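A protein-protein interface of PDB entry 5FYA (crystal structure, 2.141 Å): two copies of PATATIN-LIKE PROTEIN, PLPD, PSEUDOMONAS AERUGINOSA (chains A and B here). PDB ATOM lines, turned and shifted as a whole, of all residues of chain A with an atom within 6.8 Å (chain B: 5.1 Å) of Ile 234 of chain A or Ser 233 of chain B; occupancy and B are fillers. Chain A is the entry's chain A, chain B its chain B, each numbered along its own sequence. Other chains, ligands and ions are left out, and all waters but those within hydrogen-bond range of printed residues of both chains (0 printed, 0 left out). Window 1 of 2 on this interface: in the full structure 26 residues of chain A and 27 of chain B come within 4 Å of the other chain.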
ATOM      1  N   ILE A 149      14.921 -28.583  12.192  1.00  0.00           N
ATOM      2  CA  ILE A 149      15.982 -27.643  12.545  1.00  0.00           C
ATOM      3  C   ILE A 149      17.329 -28.346  12.761  1.00  0.00           C
ATOM      4  O   ILE A 149      18.379 -27.714  12.729  1.00  0.00           O
ATOM      5  CB  ILE A 149      15.593 -26.776  13.774  1.00  0.00           C
ATOM      6  CG1 ILE A 149      16.552 -25.594  13.949  1.00  0.00           C
ATOM      7  CG2 ILE A 149      15.516 -27.626  15.037  1.00  0.00           C
ATOM      8  CD1 ILE A 149      16.621 -24.672  12.753  1.00  0.00           C
ATOM      9  N   ILE A 172       7.773 -19.860  14.523  1.00  0.00           N
ATOM     10  CA  ILE A 172       8.801 -18.881  14.194  1.00  0.00           C
ATOM     11  C   ILE A 172       9.854 -18.838  15.290  1.00  0.00           C
ATOM     12  O   ILE A 172       9.525 -18.622  16.453  1.00  0.00           O
ATOM     13  CB  ILE A 172       8.194 -17.472  14.051  1.00  0.00           C
ATOM     14  CG1 ILE A 172       7.097 -17.469  12.986  1.00  0.00           C
ATOM     15  CG2 ILE A 172       9.269 -16.450  13.716  1.00  0.00           C
ATOM     16  CD1 ILE A 172       6.364 -16.150  12.875  1.00  0.00           C
ATOM     17  N   PRO A 173      11.126 -19.058  14.924  1.00  0.00           N
ATOM     18  CA  PRO A 173      12.228 -18.963  15.888  1.00  0.00           C
ATOM     19  C   PRO A 173      12.210 -17.610  16.590  1.00  0.00           C
ATOM     20  O   PRO A 173      11.792 -16.619  15.990  1.00  0.00           O
ATOM     21  CB  PRO A 173      13.471 -19.085  15.004  1.00  0.00           C
ATOM     22  CG  PRO A 173      13.007 -19.865  13.819  1.00  0.00           C
ATOM     23  CD  PRO A 173      11.601 -19.408  13.574  1.00  0.00           C
ATOM     24  N   ASP A 188       9.258 -23.295  11.915  1.00  0.00           N
ATOM     25  CA  ASP A 188       8.383 -22.959  10.795  1.00  0.00           C
ATOM     26  C   ASP A 188       9.041 -23.273   9.452  1.00  0.00           C
ATOM     27  O   ASP A 188      10.270 -23.321   9.347  1.00  0.00           O
ATOM     28  CB  ASP A 188       7.894 -21.505  10.865  1.00  0.00           C
ATOM     29  CG  ASP A 188       9.016 -20.491  10.767  1.00  0.00           C
ATOM     30  OD1 ASP A 188      10.188 -20.893  10.637  1.00  0.00           O
ATOM     31  OD2 ASP A 188       8.717 -19.279  10.810  1.00  0.00           O
ATOM     32  N   GLY A 190       9.144 -21.629   6.732  1.00  0.00           N
ATOM     33  CA  GLY A 190       9.479 -20.458   5.943  1.00  0.00           C
ATOM     34  C   GLY A 190      10.870 -20.467   5.342  1.00  0.00           C
ATOM     35  O   GLY A 190      11.075 -20.013   4.215  1.00  0.00           O
ATOM     36  N   MET A 191      11.831 -21.001   6.084  1.00  0.00           N
ATOM     37  CA  MET A 191      13.210 -20.976   5.627  1.00  0.00           C
ATOM     38  C   MET A 191      13.538 -22.059   4.598  1.00  0.00           C
ATOM     39  O   MET A 191      14.618 -22.030   4.007  1.00  0.00           O
ATOM     40  CB  MET A 191      14.174 -21.055   6.811  1.00  0.00           C
ATOM     41  CG  MET A 191      14.198 -22.396   7.506  1.00  0.00           C
ATOM     42  SD  MET A 191      15.334 -22.364   8.902  1.00  0.00           S
ATOM     43  CE  MET A 191      14.518 -21.160   9.958  1.00  0.00           C
ATOM     44  N   VAL A 229      19.286  -8.786  13.196  1.00  0.00           N
ATOM     45  CA  VAL A 229      20.216  -9.312  12.203  1.00  0.00           C
ATOM     46  C   VAL A 229      19.882 -10.764  11.860  1.00  0.00           C
ATOM     47  O   VAL A 229      19.817 -11.143  10.679  1.00  0.00           O
ATOM     48  CB  VAL A 229      21.674  -9.208  12.692  1.00  0.00           C
ATOM     49  CG1 VAL A 229      22.625  -9.826  11.680  1.00  0.00           C
ATOM     50  CG2 VAL A 229      22.042  -7.757  12.951  1.00  0.00           C
ATOM     51  N   MET A 230      19.654 -11.567  12.898  1.00  0.00           N
ATOM     52  CA  MET A 230      19.300 -12.971  12.719  1.00  0.00           C
ATOM     53  C   MET A 230      18.018 -13.118  11.904  1.00  0.00           C
ATOM     54  O   MET A 230      17.963 -13.864  10.911  1.00  0.00           O
ATOM     55  CB  MET A 230      19.122 -13.641  14.079  1.00  0.00           C
ATOM     56  CG  MET A 230      20.327 -13.517  14.982  1.00  0.00           C
ATOM     57  SD  MET A 230      21.784 -14.270  14.252  1.00  0.00           S
ATOM     58  CE  MET A 230      22.187 -15.458  15.527  1.00  0.00           C
ATOM     59  N   ASN A 231      16.989 -12.394  12.334  1.00  0.00           N
ATOM     60  CA  ASN A 231      15.707 -12.402  11.649  1.00  0.00           C
ATOM     61  C   ASN A 231      15.818 -11.952  10.204  1.00  0.00           C
ATOM     62  O   ASN A 231      15.127 -12.473   9.329  1.00  0.00           O
ATOM     63  CB  ASN A 231      14.699 -11.530  12.389  1.00  0.00           C
ATOM     64  CG  ASN A 231      14.073 -12.246  13.561  1.00  0.00           C
ATOM     65  OD1 ASN A 231      13.996 -13.474  13.580  1.00  0.00           O
ATOM     66  ND2 ASN A 231      13.616 -11.484  14.548  1.00  0.00           N
ATOM     67  N   GLN A 232      16.696 -10.985   9.958  1.00  0.00           N
ATOM     68  CA  GLN A 232      16.926 -10.498   8.606  1.00  0.00           C
ATOM     69  C   GLN A 232      17.529 -11.605   7.750  1.00  0.00           C
ATOM     70  O   GLN A 232      17.123 -11.804   6.602  1.00  0.00           O
ATOM     71  CB  GLN A 232      17.843  -9.280   8.623  1.00  0.00           C
ATOM     72  CG  GLN A 232      18.080  -8.665   7.255  1.00  0.00           C
ATOM     73  CD  GLN A 232      16.966  -7.730   6.827  1.00  0.00           C
ATOM     74  OE1 GLN A 232      15.863  -7.765   7.370  1.00  0.00           O
ATOM     75  NE2 GLN A 232      17.258  -6.877   5.853  1.00  0.00           N
ATOM     76  N   SER A 233      18.494 -12.325   8.319  1.00  0.00           N
ATOM     77  CA  SER A 233      19.119 -13.451   7.627  1.00  0.00           C
ATOM     78  C   SER A 233      18.068 -14.484   7.217  1.00  0.00           C
ATOM     79  O   SER A 233      17.992 -14.916   6.048  1.00  0.00           O
ATOM     80  CB  SER A 233      20.169 -14.096   8.533  1.00  0.00           C
ATOM     81  OG  SER A 233      20.855 -15.139   7.866  1.00  0.00           O
ATOM     82  N   ILE A 234      17.248 -14.865   8.191  1.00  0.00           N
ATOM     83  CA  ILE A 234      16.132 -15.771   7.938  1.00  0.00           C
ATOM     84  C   ILE A 234      15.199 -15.243   6.833  1.00  0.00           C
ATOM     85  O   ILE A 234      14.738 -16.005   5.971  1.00  0.00           O
ATOM     86  CB  ILE A 234      15.350 -16.041   9.240  1.00  0.00           C
ATOM     87  CG1 ILE A 234      16.213 -16.865  10.200  1.00  0.00           C
ATOM     88  CG2 ILE A 234      14.025 -16.737   8.957  1.00  0.00           C
ATOM     89  CD1 ILE A 234      15.538 -17.179  11.524  1.00  0.00           C
ATOM     90  N   THR A 235      14.940 -13.937   6.854  1.00  0.00           N
ATOM     91  CA  THR A 235      14.127 -13.301   5.823  1.00  0.00           C
ATOM     92  C   THR A 235      14.737 -13.498   4.435  1.00  0.00           C
ATOM     93  O   THR A 235      14.036 -13.853   3.492  1.00  0.00           O
ATOM     94  CB  THR A 235      13.929 -11.798   6.098  1.00  0.00           C
ATOM     95  OG1 THR A 235      13.226 -11.628   7.334  1.00  0.00           O
ATOM     96  CG2 THR A 235      13.131 -11.144   4.977  1.00  0.00           C
ATOM     97  N   LEU A 236      16.044 -13.278   4.320  1.00  0.00           N
ATOM     98  CA  LEU A 236      16.761 -13.507   3.064  1.00  0.00           C
ATOM     99  C   LEU A 236      16.577 -14.938   2.544  1.00  0.00           C
ATOM    100  O   LEU A 236      16.207 -15.158   1.379  1.00  0.00           O
ATOM    101  CB  LEU A 236      18.243 -13.223   3.262  1.00  0.00           C
ATOM    102  CG  LEU A 236      18.614 -11.752   3.447  1.00  0.00           C
ATOM    103  CD1 LEU A 236      20.044 -11.612   3.950  1.00  0.00           C
ATOM    104  CD2 LEU A 236      18.427 -11.013   2.130  1.00  0.00           C
ATOM    105  N   MET A 237      16.849 -15.901   3.418  1.00  0.00           N
ATOM    106  CA  MET A 237      16.632 -17.317   3.127  1.00  0.00           C
ATOM    107  C   MET A 237      15.239 -17.575   2.530  1.00  0.00           C
ATOM    108  O   MET A 237      15.066 -18.173   1.437  1.00  0.00           O
ATOM    109  CB  MET A 237      16.736 -18.066   4.451  1.00  0.00           C
ATOM    110  CG  MET A 237      17.288 -19.459   4.390  1.00  0.00           C
ATOM    111  SD  MET A 237      17.543 -20.043   6.075  1.00  0.00           S
ATOM    112  CE  MET A 237      18.375 -21.584   5.737  1.00  0.00           C
ATOM    113  N   THR A 238      14.251 -17.100   3.280  1.00  0.00           N
ATOM    114  CA  THR A 238      12.843 -17.265   2.957  1.00  0.00           C
ATOM    115  C   THR A 238      12.506 -16.688   1.588  1.00  0.00           C
ATOM    116  O   THR A 238      11.797 -17.313   0.787  1.00  0.00           O
ATOM    117  CB  THR A 238      11.998 -16.570   4.026  1.00  0.00           C
ATOM    118  OG1 THR A 238      12.356 -17.092   5.309  1.00  0.00           O
ATOM    119  CG2 THR A 238      10.520 -16.790   3.786  1.00  0.00           C
ATOM    120  N   ARG A 239      13.032 -15.495   1.329  1.00  0.00           N
ATOM    121  CA  ARG A 239      12.813 -14.807   0.069  1.00  0.00           C
ATOM    122  C   ARG A 239      13.404 -15.593  -1.088  1.00  0.00           C
ATOM    123  O   ARG A 239      12.798 -15.678  -2.155  1.00  0.00           O
ATOM    124  CB  ARG A 239      13.421 -13.403   0.111  1.00  0.00           C
ATOM    125  CG  ARG A 239      12.666 -12.439   1.010  1.00  0.00           C
ATOM    126  CD  ARG A 239      13.453 -11.158   1.227  1.00  0.00           C
ATOM    127  NE  ARG A 239      13.715 -10.458  -0.026  1.00  0.00           N
ATOM    128  CZ  ARG A 239      12.926  -9.517  -0.534  1.00  0.00           C
ATOM    129  NH1 ARG A 239      11.820  -9.161   0.105  1.00  0.00           N
ATOM    130  NH2 ARG A 239      13.244  -8.931  -1.681  1.00  0.00           N
ATOM    131  N   ASN A 241      13.970 -19.000  -1.307  1.00  0.00           N
ATOM    132  CA  ASN A 241      13.150 -20.174  -1.647  1.00  0.00           C
ATOM    133  C   ASN A 241      11.771 -19.797  -2.224  1.00  0.00           C
ATOM    134  O   ASN A 241      11.219 -20.500  -3.097  1.00  0.00           O
ATOM    135  CB  ASN A 241      13.062 -21.198  -0.493  1.00  0.00           C
ATOM    136  CG  ASN A 241      12.042 -20.823   0.565  1.00  0.00           C
ATOM    137  OD1 ASN A 241      10.835 -20.859   0.321  1.00  0.00           O
ATOM    138  ND2 ASN A 241      12.522 -20.500   1.763  1.00  0.00           N
ATOM    139  N   VAL B 229      19.336 -21.958  17.464  1.00  0.00           N
ATOM    140  CA  VAL B 229      18.423 -22.165  16.341  1.00  0.00           C
ATOM    141  C   VAL B 229      18.715 -21.189  15.197  1.00  0.00           C
ATOM    142  O   VAL B 229      18.838 -21.589  14.025  1.00  0.00           O
ATOM    143  CB  VAL B 229      16.954 -22.027  16.791  1.00  0.00           C
ATOM    144  CG1 VAL B 229      16.018 -22.093  15.595  1.00  0.00           C
ATOM    145  CG2 VAL B 229      16.606 -23.110  17.803  1.00  0.00           C
ATOM    146  N   MET B 230      18.830 -19.912  15.548  1.00  0.00           N
ATOM    147  CA  MET B 230      19.156 -18.872  14.574  1.00  0.00           C
ATOM    148  C   MET B 230      20.455 -19.198  13.839  1.00  0.00           C
ATOM    149  O   MET B 230      20.523 -19.184  12.596  1.00  0.00           O
ATOM    150  CB  MET B 230      19.299 -17.533  15.286  1.00  0.00           C
ATOM    151  CG  MET B 230      18.135 -17.192  16.187  1.00  0.00           C
ATOM    152  SD  MET B 230      16.629 -16.922  15.255  1.00  0.00           S
ATOM    153  CE  MET B 230      16.315 -15.205  15.645  1.00  0.00           C
ATOM    154  N   ASN B 231      21.486 -19.496  14.623  1.00  0.00           N
ATOM    155  CA  ASN B 231      22.781 -19.880  14.078  1.00  0.00           C
ATOM    156  C   ASN B 231      22.692 -21.097  13.171  1.00  0.00           C
ATOM    157  O   ASN B 231      23.385 -21.176  12.157  1.00  0.00           O
ATOM    158  CB  ASN B 231      23.781 -20.133  15.202  1.00  0.00           C
ATOM    159  CG  ASN B 231      24.360 -18.855  15.756  1.00  0.00           C
ATOM    160  OD1 ASN B 231      24.337 -17.818  15.096  1.00  0.00           O
ATOM    161  ND2 ASN B 231      24.894 -18.919  16.970  1.00  0.00           N
ATOM    162  N   GLN B 232      21.835 -22.045  13.538  1.00  0.00           N
ATOM    163  CA  GLN B 232      21.633 -23.233  12.723  1.00  0.00           C
ATOM    164  C   GLN B 232      21.073 -22.856  11.355  1.00  0.00           C
ATOM    165  O   GLN B 232      21.513 -23.383  10.324  1.00  0.00           O
ATOM    166  CB  GLN B 232      20.690 -24.211  13.422  1.00  0.00           C
ATOM    167  CG  GLN B 232      20.533 -25.528  12.692  1.00  0.00           C
ATOM    168  CD  GLN B 232      21.512 -26.580  13.170  1.00  0.00           C
ATOM    169  OE1 GLN B 232      22.680 -26.291  13.418  1.00  0.00           O
ATOM    170  NE2 GLN B 232      21.033 -27.810  13.314  1.00  0.00           N
ATOM    171  N   SER B 233      20.108 -21.938  11.341  1.00  0.00           N
ATOM    172  CA  SER B 233      19.530 -21.497  10.070  1.00  0.00           C
ATOM    173  C   SER B 233      20.574 -20.798   9.192  1.00  0.00           C
ATOM    174  O   SER B 233      20.669 -21.041   7.969  1.00  0.00           O
ATOM    175  CB  SER B 233      18.328 -20.582  10.309  1.00  0.00           C
ATOM    176  OG  SER B 233      18.703 -19.433  11.042  1.00  0.00           O
ATOM    177  N   ILE B 234      21.366 -19.934   9.824  1.00  0.00           N
ATOM    178  CA  ILE B 234      22.454 -19.273   9.114  1.00  0.00           C
ATOM    179  C   ILE B 234      23.408 -20.308   8.515  1.00  0.00           C
ATOM    180  O   ILE B 234      23.857 -20.179   7.365  1.00  0.00           O
ATOM    181  CB  ILE B 234      23.217 -18.306  10.038  1.00  0.00           C
ATOM    182  CG1 ILE B 234      22.355 -17.074  10.326  1.00  0.00           C
ATOM    183  CG2 ILE B 234      24.540 -17.902   9.415  1.00  0.00           C
ATOM    184  CD1 ILE B 234      23.010 -16.068  11.252  1.00  0.00           C
ATOM    185  N   THR B 235      23.689 -21.349   9.294  1.00  0.00           N
ATOM    186  CA  THR B 235      24.560 -22.429   8.850  1.00  0.00           C
ATOM    187  C   THR B 235      23.983 -23.108   7.614  1.00  0.00           C
ATOM    188  O   THR B 235      24.712 -23.421   6.664  1.00  0.00           O
ATOM    189  CB  THR B 235      24.786 -23.460   9.969  1.00  0.00           C
ATOM    190  OG1 THR B 235      25.428 -22.823  11.079  1.00  0.00           O
ATOM    191  CG2 THR B 235      25.666 -24.591   9.480  1.00  0.00           C
ATOM    192  N   LEU B 236      22.670 -23.312   7.617  1.00  0.00           N
ATOM    193  CA  LEU B 236      21.994 -23.890   6.456  1.00  0.00           C
ATOM    194  C   LEU B 236      22.145 -23.051   5.182  1.00  0.00           C
ATOM    195  O   LEU B 236      22.548 -23.578   4.133  1.00  0.00           O
ATOM    196  CB  LEU B 236      20.522 -24.120   6.757  1.00  0.00           C
ATOM    197  CG  LEU B 236      20.228 -25.242   7.746  1.00  0.00           C
ATOM    198  CD1 LEU B 236      18.795 -25.133   8.244  1.00  0.00           C
ATOM    199  CD2 LEU B 236      20.473 -26.584   7.072  1.00  0.00           C
ATOM    200  N   MET B 237      21.827 -21.759   5.256  1.00  0.00           N
ATOM    201  CA  MET B 237      21.938 -20.931   4.048  1.00  0.00           C
ATOM    202  C   MET B 237      23.397 -20.846   3.568  1.00  0.00           C
ATOM    203  O   MET B 237      23.687 -20.837   2.351  1.00  0.00           O
ATOM    204  CB  MET B 237      21.308 -19.540   4.242  1.00  0.00           C
ATOM    205  CG  MET B 237      22.110 -18.554   5.079  1.00  0.00           C
ATOM    206  SD  MET B 237      21.195 -17.039   5.472  1.00  0.00           S
ATOM    207  CE  MET B 237      20.621 -16.535   3.853  1.00  0.00           C
ATOM    208  N   THR B 238      24.308 -20.821   4.536  1.00  0.00           N
ATOM    209  CA  THR B 238      25.736 -20.827   4.253  1.00  0.00           C
ATOM    210  C   THR B 238      26.127 -22.072   3.455  1.00  0.00           C
ATOM    211  O   THR B 238      26.861 -21.990   2.460  1.00  0.00           O
ATOM    212  CB  THR B 238      26.547 -20.768   5.554  1.00  0.00           C
ATOM    213  OG1 THR B 238      26.319 -19.506   6.191  1.00  0.00           O
ATOM    214  CG2 THR B 238      28.029 -20.931   5.277  1.00  0.00           C
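Of the printed residues of chain B, Ile 234 of chain A touches Met 230 (3.9 Å) and Ser 233 (3.7 Å).
Ser 233 of chain B touches just these residues of chain A: Met 191 (3.8 Å), Ile 234 (3.7 Å) and Met 237 (3.2 Å).
Of the printed residues of chain B, Asn 231 of chain A touches Met 230 (3.6 Å).
Of the printed residues of chain A, Val 229 of chain B touches Ile 149 (3.9 Å) and Pro 173 (3.99 Å).
Of the printed residues of chain B, Ser 233 of chain A touches Ile 234 (3.5 Å) and Met 237 (3.1 Å).
Of the printed residues of chain A, Met 230 of chain B touches Pro 173, Met 230, Asn 231 and Ile 234.
Gly 190 of chain A touches none of the printed residues of chain B.
Asn 241 of chain A touches none of the printed residues of chain B.
The nearest printed residue of chain B that does not touch Met 237 of chain A is Ile 234 of chain B (5.3 Å).
O of Ile 149 of chain A lies within hydrogen-bond range of NE2 of Gln 232 of chain B (2.7 Å).
The side-chain hydroxyl (OG) of Ser 233 of chain A lies within hydrogen-bond range of the side-chain sulfur (SD) of Met 237 of chain B (3.1 Å).
O of Ser 233 of chain B sits close to SD of Met 237 of chain A, at 3.8 Å.
Hydrophobic or aromatic side chains of chain A that line the printed part of chain B: Ile 149, Pro 173, Met 191, Met 230, Ile 234 and Met 237.
Among the printed residues, no Asp or Glu carboxylate lies within 4 Å of a Lys or Arg side-chain nitrogen of the other chain.
The side-chain amide nitrogen of Asn 241 of chain A lies close to the backbone carbonyl oxygen of Met 191 of chain A, at 3.4 Å.
O of Asn 231 of chain A lies within hydrogen-bond range of OG1 of Thr 235 of chain A, 2.9 Å away.
ND2 of Asn 241 of chain A lies within hydrogen-bond range of O of Met 237 of chain A (3.5 Å).
O of Met 230 of chain B sits at hydrogen-bond distance from OG of Ser 233 of chain B, 2.4 Å away.
O of Asn 231 of chain B sits at hydrogen-bond distance from OG1 of Thr 235 of chain B (2.8 Å).
OG1 of Thr 238 of chain B is in hydrogen-bond range of O of Ile 234 of chain B, at 2.8 Å.
Met 230 of chain A touches Ile 234 of chain B, and with the chains exchanged Ile 234 of chain A touches Met 230 of chain B.
Ser 233 of chain A touches Ile 234 of chain B, and with the chains exchanged Ile 234 of chain A touches Ser 233 of chain B.
Ser 233 of chain A touches Met 237 of chain B, and with the chains exchanged Met 237 of chain A touches Ser 233 of chain B.
Met 237 of chain A touches Leu 236 of chain B, but with the chains exchanged Leu 236 of chain A does not touch Met 237 of chain B (4.1 Å).
Of the 16 pairs that touch across the chains among the printed residues, 10 have their exchanged pair printed and touching as well.
Ile 149 of chain A touches Val 229 of chain B.
Pro 173 of chain A touches Met 230 of chain B.
Ser 233 of chain B touches Met 191 of chain A.
Met 230 of chain A touches Met 230 of chain B (CE to CB, 3.6 Å).
SD of Met 230 of chain A touches CD1 of Ile 234 of chain B (3.7 Å).
Met 230 of chain B touches Asn 231 of chain A (CE to OD1, 3.6 Å).
Ser 233 of chain A touches Ile 234 of chain B (OG to CG1, 3.5 Å).
Met 230 of chain B touches Ile 234 of chain A.
Ser 233 of chain B touches Ile 234 of chain A (OG to CG1, 3.7 Å).
CE of Met 237 of chain A touches N of Met 237 of chain B (3.5 Å).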
